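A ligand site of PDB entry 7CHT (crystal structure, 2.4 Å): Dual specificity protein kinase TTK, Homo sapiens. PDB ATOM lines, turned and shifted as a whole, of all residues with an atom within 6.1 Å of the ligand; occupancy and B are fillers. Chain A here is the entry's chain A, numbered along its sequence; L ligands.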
ATOM      1  N   LYS A  15     -13.282  33.390  22.523  1.00  0.00           N
ATOM      2  CA  LYS A  15     -12.723  33.259  21.176  1.00  0.00           C
ATOM      3  C   LYS A  15     -13.825  32.820  20.222  1.00  0.00           C
ATOM      4  O   LYS A  15     -14.899  32.373  20.645  1.00  0.00           O
ATOM      5  CB  LYS A  15     -11.568  32.261  21.132  1.00  0.00           C
ATOM      6  CG  LYS A  15     -11.989  30.815  21.327  1.00  0.00           C
ATOM      7  CD  LYS A  15     -10.892  29.859  20.952  1.00  0.00           C
ATOM      8  CE  LYS A  15     -11.154  28.497  21.559  1.00  0.00           C
ATOM      9  NZ  LYS A  15     -10.335  27.469  20.871  1.00  0.00           N
ATOM     10  N   ILE A  17     -14.959  30.151  17.698  1.00  0.00           N
ATOM     11  CA  ILE A  17     -14.732  28.760  17.336  1.00  0.00           C
ATOM     12  C   ILE A  17     -14.801  28.579  15.826  1.00  0.00           C
ATOM     13  O   ILE A  17     -13.980  27.879  15.234  1.00  0.00           O
ATOM     14  CB  ILE A  17     -15.750  27.859  18.046  1.00  0.00           C
ATOM     15  CG1 ILE A  17     -15.577  27.932  19.552  1.00  0.00           C
ATOM     16  CG2 ILE A  17     -15.645  26.449  17.508  1.00  0.00           C
ATOM     17  CD1 ILE A  17     -16.789  27.471  20.334  1.00  0.00           C
ATOM     18  N   GLY A  18     -15.815  29.162  15.185  1.00  0.00           N
ATOM     19  CA  GLY A  18     -15.973  28.910  13.762  1.00  0.00           C
ATOM     20  C   GLY A  18     -16.877  29.935  13.107  1.00  0.00           C
ATOM     21  O   GLY A  18     -17.429  30.834  13.750  1.00  0.00           O
ATOM     22  N   SER A  19     -17.040  29.761  11.800  1.00  0.00           N
ATOM     23  CA  SER A  19     -17.868  30.664  11.020  1.00  0.00           C
ATOM     24  C   SER A  19     -18.317  29.914   9.780  1.00  0.00           C
ATOM     25  O   SER A  19     -17.782  28.850   9.443  1.00  0.00           O
ATOM     26  CB  SER A  19     -17.110  31.950  10.672  1.00  0.00           C
ATOM     27  OG  SER A  19     -15.916  31.666   9.963  1.00  0.00           O
ATOM     28  N   VAL A  25     -19.669  31.165  15.626  1.00  0.00           N
ATOM     29  CA  VAL A  25     -19.835  30.525  16.927  1.00  0.00           C
ATOM     30  C   VAL A  25     -18.692  30.984  17.824  1.00  0.00           C
ATOM     31  O   VAL A  25     -17.522  30.930  17.422  1.00  0.00           O
ATOM     32  CB  VAL A  25     -19.876  28.999  16.822  1.00  0.00           C
ATOM     33  CG1 VAL A  25     -20.248  28.382  18.145  1.00  0.00           C
ATOM     34  CG2 VAL A  25     -20.841  28.570  15.782  1.00  0.00           C
ATOM     35  N   GLN A  27     -16.884  30.868  21.753  1.00  0.00           N
ATOM     36  CA  GLN A  27     -16.773  30.301  23.081  1.00  0.00           C
ATOM     37  C   GLN A  27     -16.791  31.472  24.069  1.00  0.00           C
ATOM     38  O   GLN A  27     -16.003  32.410  23.921  1.00  0.00           O
ATOM     39  CB  GLN A  27     -15.490  29.475  23.198  1.00  0.00           C
ATOM     40  CG  GLN A  27     -15.148  29.087  24.590  1.00  0.00           C
ATOM     41  CD  GLN A  27     -13.809  28.342  24.657  1.00  0.00           C
ATOM     42  OE1 GLN A  27     -12.827  28.744  24.019  1.00  0.00           O
ATOM     43  NE2 GLN A  27     -13.785  27.251  25.387  1.00  0.00           N
ATOM     44  N   ILE A  35     -18.731  28.378  31.172  1.00  0.00           N
ATOM     45  CA  ILE A  35     -18.433  28.396  29.749  1.00  0.00           C
ATOM     46  C   ILE A  35     -19.663  27.952  28.961  1.00  0.00           C
ATOM     47  O   ILE A  35     -20.485  27.154  29.426  1.00  0.00           O
ATOM     48  CB  ILE A  35     -17.213  27.526  29.436  1.00  0.00           C
ATOM     49  CG1 ILE A  35     -16.677  27.856  28.036  1.00  0.00           C
ATOM     50  CG2 ILE A  35     -17.570  26.052  29.505  1.00  0.00           C
ATOM     51  CD1 ILE A  35     -15.665  26.845  27.539  1.00  0.00           C
ATOM     52  N   ALA A  37     -21.338  28.068  24.521  1.00  0.00           N
ATOM     53  CA  ALA A  37     -21.173  28.433  23.120  1.00  0.00           C
ATOM     54  C   ALA A  37     -22.319  29.347  22.702  1.00  0.00           C
ATOM     55  O   ALA A  37     -23.479  29.146  23.087  1.00  0.00           O
ATOM     56  CB  ALA A  37     -21.104  27.176  22.225  1.00  0.00           C
ATOM     57  N   LYS A  39     -23.937  30.924  19.141  1.00  0.00           N
ATOM     58  CA  LYS A  39     -24.005  31.012  17.680  1.00  0.00           C
ATOM     59  C   LYS A  39     -24.728  32.306  17.295  1.00  0.00           C
ATOM     60  O   LYS A  39     -25.787  32.636  17.853  1.00  0.00           O
ATOM     61  CB  LYS A  39     -24.717  29.778  17.103  1.00  0.00           C
ATOM     62  CG  LYS A  39     -24.772  29.677  15.587  1.00  0.00           C
ATOM     63  CD  LYS A  39     -25.292  28.301  15.158  1.00  0.00           C
ATOM     64  CE  LYS A  39     -25.456  28.218  13.647  1.00  0.00           C
ATOM     65  NZ  LYS A  39     -25.884  26.865  13.185  1.00  0.00           N
ATOM     66  N   GLU A  57     -34.076  24.782  12.238  1.00  0.00           N
ATOM     67  CA  GLU A  57     -33.046  24.288  13.147  1.00  0.00           C
ATOM     68  C   GLU A  57     -33.391  24.617  14.606  1.00  0.00           C
ATOM     69  O   GLU A  57     -33.331  23.736  15.477  1.00  0.00           O
ATOM     70  CB  GLU A  57     -31.671  24.883  12.790  1.00  0.00           C
ATOM     71  CG  GLU A  57     -30.469  24.030  13.309  1.00  0.00           C
ATOM     72  CD  GLU A  57     -29.130  24.798  13.340  1.00  0.00           C
ATOM     73  OE1 GLU A  57     -28.960  25.737  12.536  1.00  0.00           O
ATOM     74  OE2 GLU A  57     -28.242  24.448  14.162  1.00  0.00           O
ATOM     75  N   ILE A  72     -26.746  18.302  21.339  1.00  0.00           N
ATOM     76  CA  ILE A  72     -26.275  19.522  21.963  1.00  0.00           C
ATOM     77  C   ILE A  72     -27.465  20.318  22.501  1.00  0.00           C
ATOM     78  O   ILE A  72     -28.489  20.466  21.824  1.00  0.00           O
ATOM     79  CB  ILE A  72     -25.475  20.366  20.958  1.00  0.00           C
ATOM     80  CG1 ILE A  72     -24.433  21.229  21.673  1.00  0.00           C
ATOM     81  CG2 ILE A  72     -26.409  21.183  20.129  1.00  0.00           C
ATOM     82  CD1 ILE A  72     -23.218  20.381  22.189  1.00  0.00           C
ATOM     83  N   MET A  88     -25.733  27.764  23.828  1.00  0.00           N
ATOM     84  CA  MET A  88     -25.693  26.301  23.767  1.00  0.00           C
ATOM     85  C   MET A  88     -24.576  25.776  24.655  1.00  0.00           C
ATOM     86  O   MET A  88     -23.624  26.490  24.988  1.00  0.00           O
ATOM     87  CB  MET A  88     -25.458  25.799  22.336  1.00  0.00           C
ATOM     88  CG  MET A  88     -26.572  26.180  21.407  1.00  0.00           C
ATOM     89  SD  MET A  88     -26.199  25.922  19.680  1.00  0.00           S
ATOM     90  CE  MET A  88     -25.146  27.315  19.345  1.00  0.00           C
ATOM     91  N   GLU A  89     -24.717  24.508  25.036  1.00  0.00           N
ATOM     92  CA  GLU A  89     -23.608  23.881  25.711  1.00  0.00           C
ATOM     93  C   GLU A  89     -22.418  23.907  24.760  1.00  0.00           C
ATOM     94  O   GLU A  89     -22.556  23.756  23.533  1.00  0.00           O
ATOM     95  CB  GLU A  89     -23.977  22.468  26.204  1.00  0.00           C
ATOM     96  CG  GLU A  89     -23.649  21.281  25.347  1.00  0.00           C
ATOM     97  CD  GLU A  89     -24.299  19.975  25.864  1.00  0.00           C
ATOM     98  OE1 GLU A  89     -23.736  19.287  26.748  1.00  0.00           O
ATOM     99  OE2 GLU A  89     -25.398  19.641  25.355  1.00  0.00           O
ATOM    100  N   CYS A  90     -21.266  24.239  25.308  1.00  0.00           N
ATOM    101  CA  CYS A  90     -20.059  24.379  24.526  1.00  0.00           C
ATOM    102  C   CYS A  90     -19.334  23.034  24.530  1.00  0.00           C
ATOM    103  O   CYS A  90     -19.180  22.412  25.594  1.00  0.00           O
ATOM    104  CB  CYS A  90     -19.176  25.485  25.099  1.00  0.00           C
ATOM    105  SG  CYS A  90     -17.733  25.756  24.012  1.00  0.00           S
ATOM    106  N   GLY A  91     -18.901  22.562  23.367  1.00  0.00           N
ATOM    107  CA  GLY A  91     -18.120  21.336  23.332  1.00  0.00           C
ATOM    108  C   GLY A  91     -16.635  21.572  23.584  1.00  0.00           C
ATOM    109  O   GLY A  91     -16.097  22.659  23.343  1.00  0.00           O
ATOM    110  N   ASN A  92     -15.943  20.564  24.107  1.00  0.00           N
ATOM    111  CA  ASN A  92     -14.478  20.619  24.153  1.00  0.00           C
ATOM    112  C   ASN A  92     -13.891  20.768  22.750  1.00  0.00           C
ATOM    113  O   ASN A  92     -12.962  21.560  22.539  1.00  0.00           O
ATOM    114  CB  ASN A  92     -13.935  19.369  24.851  1.00  0.00           C
ATOM    115  CG  ASN A  92     -14.712  19.021  26.111  1.00  0.00           C
ATOM    116  OD1 ASN A  92     -15.314  19.895  26.731  1.00  0.00           O
ATOM    117  ND2 ASN A  92     -14.713  17.755  26.482  1.00  0.00           N
ATOM    118  N   ILE A  93     -14.441  20.062  21.769  1.00  0.00           N
ATOM    119  CA  ILE A  93     -13.881  20.087  20.427  1.00  0.00           C
ATOM    120  C   ILE A  93     -14.805  19.252  19.561  1.00  0.00           C
ATOM    121  O   ILE A  93     -15.592  18.449  20.077  1.00  0.00           O
ATOM    122  CB  ILE A  93     -12.447  19.530  20.419  1.00  0.00           C
ATOM    123  CG1 ILE A  93     -11.783  19.730  19.058  1.00  0.00           C
ATOM    124  CG2 ILE A  93     -12.444  18.045  20.829  1.00  0.00           C
ATOM    125  CD1 ILE A  93     -10.319  19.305  19.053  1.00  0.00           C
ATOM    126  N   ASP A  94     -14.722  19.416  18.246  1.00  0.00           N
ATOM    127  CA  ASP A  94     -15.523  18.566  17.372  1.00  0.00           C
ATOM    128  C   ASP A  94     -14.767  17.300  17.022  1.00  0.00           C
ATOM    129  O   ASP A  94     -13.540  17.254  17.084  1.00  0.00           O
ATOM    130  CB  ASP A  94     -15.905  19.271  16.086  1.00  0.00           C
ATOM    131  CG  ASP A  94     -14.707  19.535  15.216  1.00  0.00           C
ATOM    132  OD1 ASP A  94     -13.848  20.336  15.649  1.00  0.00           O
ATOM    133  OD2 ASP A  94     -14.622  18.959  14.112  1.00  0.00           O
ATOM    134  N   SER A  97     -11.852  17.418  14.081  1.00  0.00           N
ATOM    135  CA  SER A  97     -10.604  17.957  14.653  1.00  0.00           C
ATOM    136  C   SER A  97      -9.943  16.984  15.611  1.00  0.00           C
ATOM    137  O   SER A  97      -8.712  16.934  15.690  1.00  0.00           O
ATOM    138  CB  SER A  97     -10.857  19.283  15.409  1.00  0.00           C
ATOM    139  OG  SER A  97     -11.491  20.262  14.582  1.00  0.00           O
ATOM    140  N   ALA A 137     -17.578  16.313  11.772  1.00  0.00           N
ATOM    141  CA  ALA A 137     -17.750  17.684  12.225  1.00  0.00           C
ATOM    142  C   ALA A 137     -19.104  17.904  12.907  1.00  0.00           C
ATOM    143  O   ALA A 137     -19.244  18.840  13.703  1.00  0.00           O
ATOM    144  CB  ALA A 137     -17.591  18.644  11.040  1.00  0.00           C
ATOM    145  N   LEU A 140     -19.805  16.710  18.605  1.00  0.00           N
ATOM    146  CA  LEU A 140     -18.924  17.374  19.535  1.00  0.00           C
ATOM    147  C   LEU A 140     -18.631  16.425  20.668  1.00  0.00           C
ATOM    148  O   LEU A 140     -19.466  15.586  21.013  1.00  0.00           O
ATOM    149  CB  LEU A 140     -19.553  18.639  20.128  1.00  0.00           C
ATOM    150  CG  LEU A 140     -19.978  19.649  19.093  1.00  0.00           C
ATOM    151  CD1 LEU A 140     -20.448  20.979  19.752  1.00  0.00           C
ATOM    152  CD2 LEU A 140     -18.822  19.874  18.144  1.00  0.00           C
ATOM    153  N   ILE A 149     -24.688  18.231  16.617  1.00  0.00           N
ATOM    154  CA  ILE A 149     -24.978  19.671  16.495  1.00  0.00           C
ATOM    155  C   ILE A 149     -25.856  19.992  15.283  1.00  0.00           C
ATOM    156  O   ILE A 149     -26.818  20.740  15.406  1.00  0.00           O
ATOM    157  CB  ILE A 149     -23.704  20.539  16.423  1.00  0.00           C
ATOM    158  CG1 ILE A 149     -22.514  20.012  17.153  1.00  0.00           C
ATOM    159  CG2 ILE A 149     -24.016  21.984  16.881  1.00  0.00           C
ATOM    160  CD1 ILE A 149     -21.335  20.907  16.773  1.00  0.00           C
ATOM    161  N   MET A 157     -20.914  25.303   9.144  1.00  0.00           N
ATOM    162  CA  MET A 157     -19.780  26.172   9.342  1.00  0.00           C
ATOM    163  C   MET A 157     -18.495  25.350   9.472  1.00  0.00           C
ATOM    164  O   MET A 157     -18.511  24.116   9.534  1.00  0.00           O
ATOM    165  CB  MET A 157     -19.989  27.007  10.603  1.00  0.00           C
ATOM    166  CG  MET A 157     -21.098  28.018  10.494  1.00  0.00           C
ATOM    167  SD  MET A 157     -21.437  28.480  12.199  1.00  0.00           S
ATOM    168  CE  MET A 157     -19.847  28.052  12.934  1.00  0.00           C
ATOM    169  N   GLN A 158     -17.391  26.067   9.532  1.00  0.00           N
ATOM    170  CA  GLN A 158     -16.055  25.483   9.588  1.00  0.00           C
ATOM    171  C   GLN A 158     -15.286  26.062  10.763  1.00  0.00           C
ATOM    172  O   GLN A 158     -15.349  27.277  11.018  1.00  0.00           O
ATOM    173  CB  GLN A 158     -15.290  25.755   8.274  1.00  0.00           C
ATOM    174  CG  GLN A 158     -16.168  25.946   7.032  1.00  0.00           C
ATOM    175  CD  GLN A 158     -16.528  27.409   6.744  1.00  0.00           C
ATOM    176  OE1 GLN A 158     -15.842  28.334   7.206  1.00  0.00           O
ATOM    177  NE2 GLN A 158     -17.608  27.612   5.987  1.00  0.00           N
ATOM    178  N   PRO A 159     -14.518  25.236  11.470  1.00  0.00           N
ATOM    179  CA  PRO A 159     -13.646  25.773  12.536  1.00  0.00           C
ATOM    180  C   PRO A 159     -12.737  26.847  11.973  1.00  0.00           C
ATOM    181  O   PRO A 159     -12.216  26.730  10.858  1.00  0.00           O
ATOM    182  CB  PRO A 159     -12.853  24.548  12.994  1.00  0.00           C
ATOM    183  CG  PRO A 159     -13.727  23.391  12.641  1.00  0.00           C
ATOM    184  CD  PRO A 159     -14.424  23.771  11.374  1.00  0.00           C
ATOM    185  N   ASP A 160     -12.558  27.911  12.750  1.00  0.00           N
ATOM    186  CA  ASP A 160     -11.657  28.979  12.319  1.00  0.00           C
ATOM    187  C   ASP A 160     -10.234  28.711  12.798  1.00  0.00           C
ATOM    188  O   ASP A 160     -10.012  27.959  13.757  1.00  0.00           O
ATOM    189  CB  ASP A 160     -12.144  30.329  12.814  1.00  0.00           C
ATOM    190  CG  ASP A 160     -13.370  30.816  12.034  1.00  0.00           C
ATOM    191  OD1 ASP A 160     -13.405  30.705  10.782  1.00  0.00           O
ATOM    192  OD2 ASP A 160     -14.315  31.294  12.693  1.00  0.00           O
HETATM  193  C1  LIG L   1     -12.213  23.267  16.590  1.00  0.00           C
HETATM  194  C2  LIG L   1     -15.755  22.946  18.804  1.00  0.00           C
HETATM  195  C3  LIG L   1     -22.062  24.717  18.751  1.00  0.00           C
HETATM  196  C4  LIG L   1     -22.643  25.099  17.395  1.00  0.00           C
HETATM  197  C5  LIG L   1     -18.318  25.250  14.883  1.00  0.00           C
HETATM  198  C6  LIG L   1     -13.712  24.912  22.556  1.00  0.00           C
HETATM  199  C7  LIG L   1     -14.725  24.215  20.561  1.00  0.00           C
HETATM  200  C8  LIG L   1     -13.549  24.294  19.833  1.00  0.00           C
HETATM  201  C9  LIG L   1     -13.495  23.678  18.597  1.00  0.00           C
HETATM  202  C10 LIG L   1     -10.888  24.243  18.206  1.00  0.00           C
HETATM  203  C11 LIG L   1      -9.982  24.003  16.933  1.00  0.00           C
HETATM  204  C12 LIG L   1     -10.567  23.128  16.232  1.00  0.00           C
HETATM  205  C13 LIG L   1     -14.596  23.030  18.076  1.00  0.00           C
HETATM  206  C14 LIG L   1     -15.822  23.559  20.044  1.00  0.00           C
HETATM  207  C15 LIG L   1     -18.330  23.826  20.157  1.00  0.00           C
HETATM  208  C16 LIG L   1     -20.620  24.130  20.354  1.00  0.00           C
HETATM  209  C17 LIG L   1     -20.700  24.449  19.011  1.00  0.00           C
HETATM  210  C18 LIG L   1     -22.760  24.561  19.935  1.00  0.00           C
HETATM  211  C19 LIG L   1     -19.498  24.419  18.258  1.00  0.00           C
HETATM  212  C20 LIG L   1     -18.322  24.399  16.067  1.00  0.00           C
HETATM  213  C21 LIG L   1     -17.120  25.034  13.962  1.00  0.00           C
HETATM  214  C22 LIG L   1     -17.153  22.730  14.585  1.00  0.00           C
HETATM  215  C23 LIG L   1     -18.267  23.002  15.628  1.00  0.00           C
HETATM  216  N1  LIG L   1     -12.306  23.701  17.781  1.00  0.00           N
HETATM  217  N2  LIG L   1     -17.058  23.501  20.801  1.00  0.00           N
HETATM  218  N3  LIG L   1     -19.412  23.815  20.889  1.00  0.00           N
HETATM  219  N4  LIG L   1     -23.052  25.393  16.382  1.00  0.00           N
HETATM  220  N5  LIG L   1     -21.873  24.209  20.893  1.00  0.00           N
HETATM  221  N6  LIG L   1     -19.498  24.702  16.850  1.00  0.00           N
HETATM  222  N7  LIG L   1     -18.349  24.108  18.872  1.00  0.00           N
HETATM  223  O1  LIG L   1     -14.869  24.814  21.806  1.00  0.00           O
HETATM  224  O2  LIG L   1     -10.589  24.729  19.261  1.00  0.00           O
HETATM  225  O3  LIG L   1     -17.104  23.669  13.456  1.00  0.00           O
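A nitrogen (N5) of the ligand lies within hydrogen-bond range of the backbone carbonyl oxygen (O) of Glu 89 (2.8 Å).
The backbone NH (N) of Gly 91 is in hydrogen-bond range of a nitrogen (N3) of the ligand (2.8 Å).
N2 of the ligand is in hydrogen-bond range of O of Gly 91 (2.8 Å).
NZ of Lys 15 lies within hydrogen-bond range of O2 of the ligand (3.2 Å).
The side-chain sulfur (SG) of Cys 90 is in hydrogen-bond range of an oxygen (O1) of the ligand (3.7 Å).
The backbone NH (N) of Gln 27 is in hydrogen-bond range of the backbone carbonyl oxygen (O) of Lys 15 (2.7 Å).
N of Met 88 is in hydrogen-bond range of O of Ala 37 (2.7 Å).
OG of Ser 97 lies within hydrogen-bond range of OD1 of Asp 94, 2.6 Å away.
The backbone carbonyl oxygen of Val 25 sits at hydrogen-bond distance from the backbone NH of Ile 17 (2.7 Å).
The backbone carbonyl oxygen (O) of Ile 17 sits at hydrogen-bond distance from the backbone NH (N) of Asp 160 (2.9 Å).
N of Gln 158 sits at hydrogen-bond distance from O of Ser 19 (2.8 Å).
OE1 of Glu 57 lies within salt-bridge range of NZ of Lys 39, 3.3 Å away.
The backbone NH of Val 25 sits at hydrogen-bond distance from the backbone carbonyl oxygen of Gly 18, 2.9 Å away.
Ile 17 touches the ligand (CD1 to O1, 3.6 Å).
Val 25 touches the ligand.
Gln 27 touches the ligand.
CB of Ala 37 touches N5 of the ligand, 3.3 Å away.
Lys 39 touches the ligand (CD to N4, 3.9 Å).
Met 88 touches the ligand.
Asn 92 touches the ligand.
Ile 93 touches the ligand (CA to C2, 3.8 Å).
Asp 94 touches the ligand.
OG of Ser 97 touches C12 of the ligand (3.4 Å).
CD1 of Leu 140 touches C16 of the ligand, at 3.2 Å.
CG2 of Ile 149 touches C4 of the ligand (3.4 Å).
Met 157 touches the ligand.
Gln 158 touches the ligand.
Pro 159 touches the ligand.
The nearest printed residue that does not touch the ligand is Ile 72 (4.01 Å).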
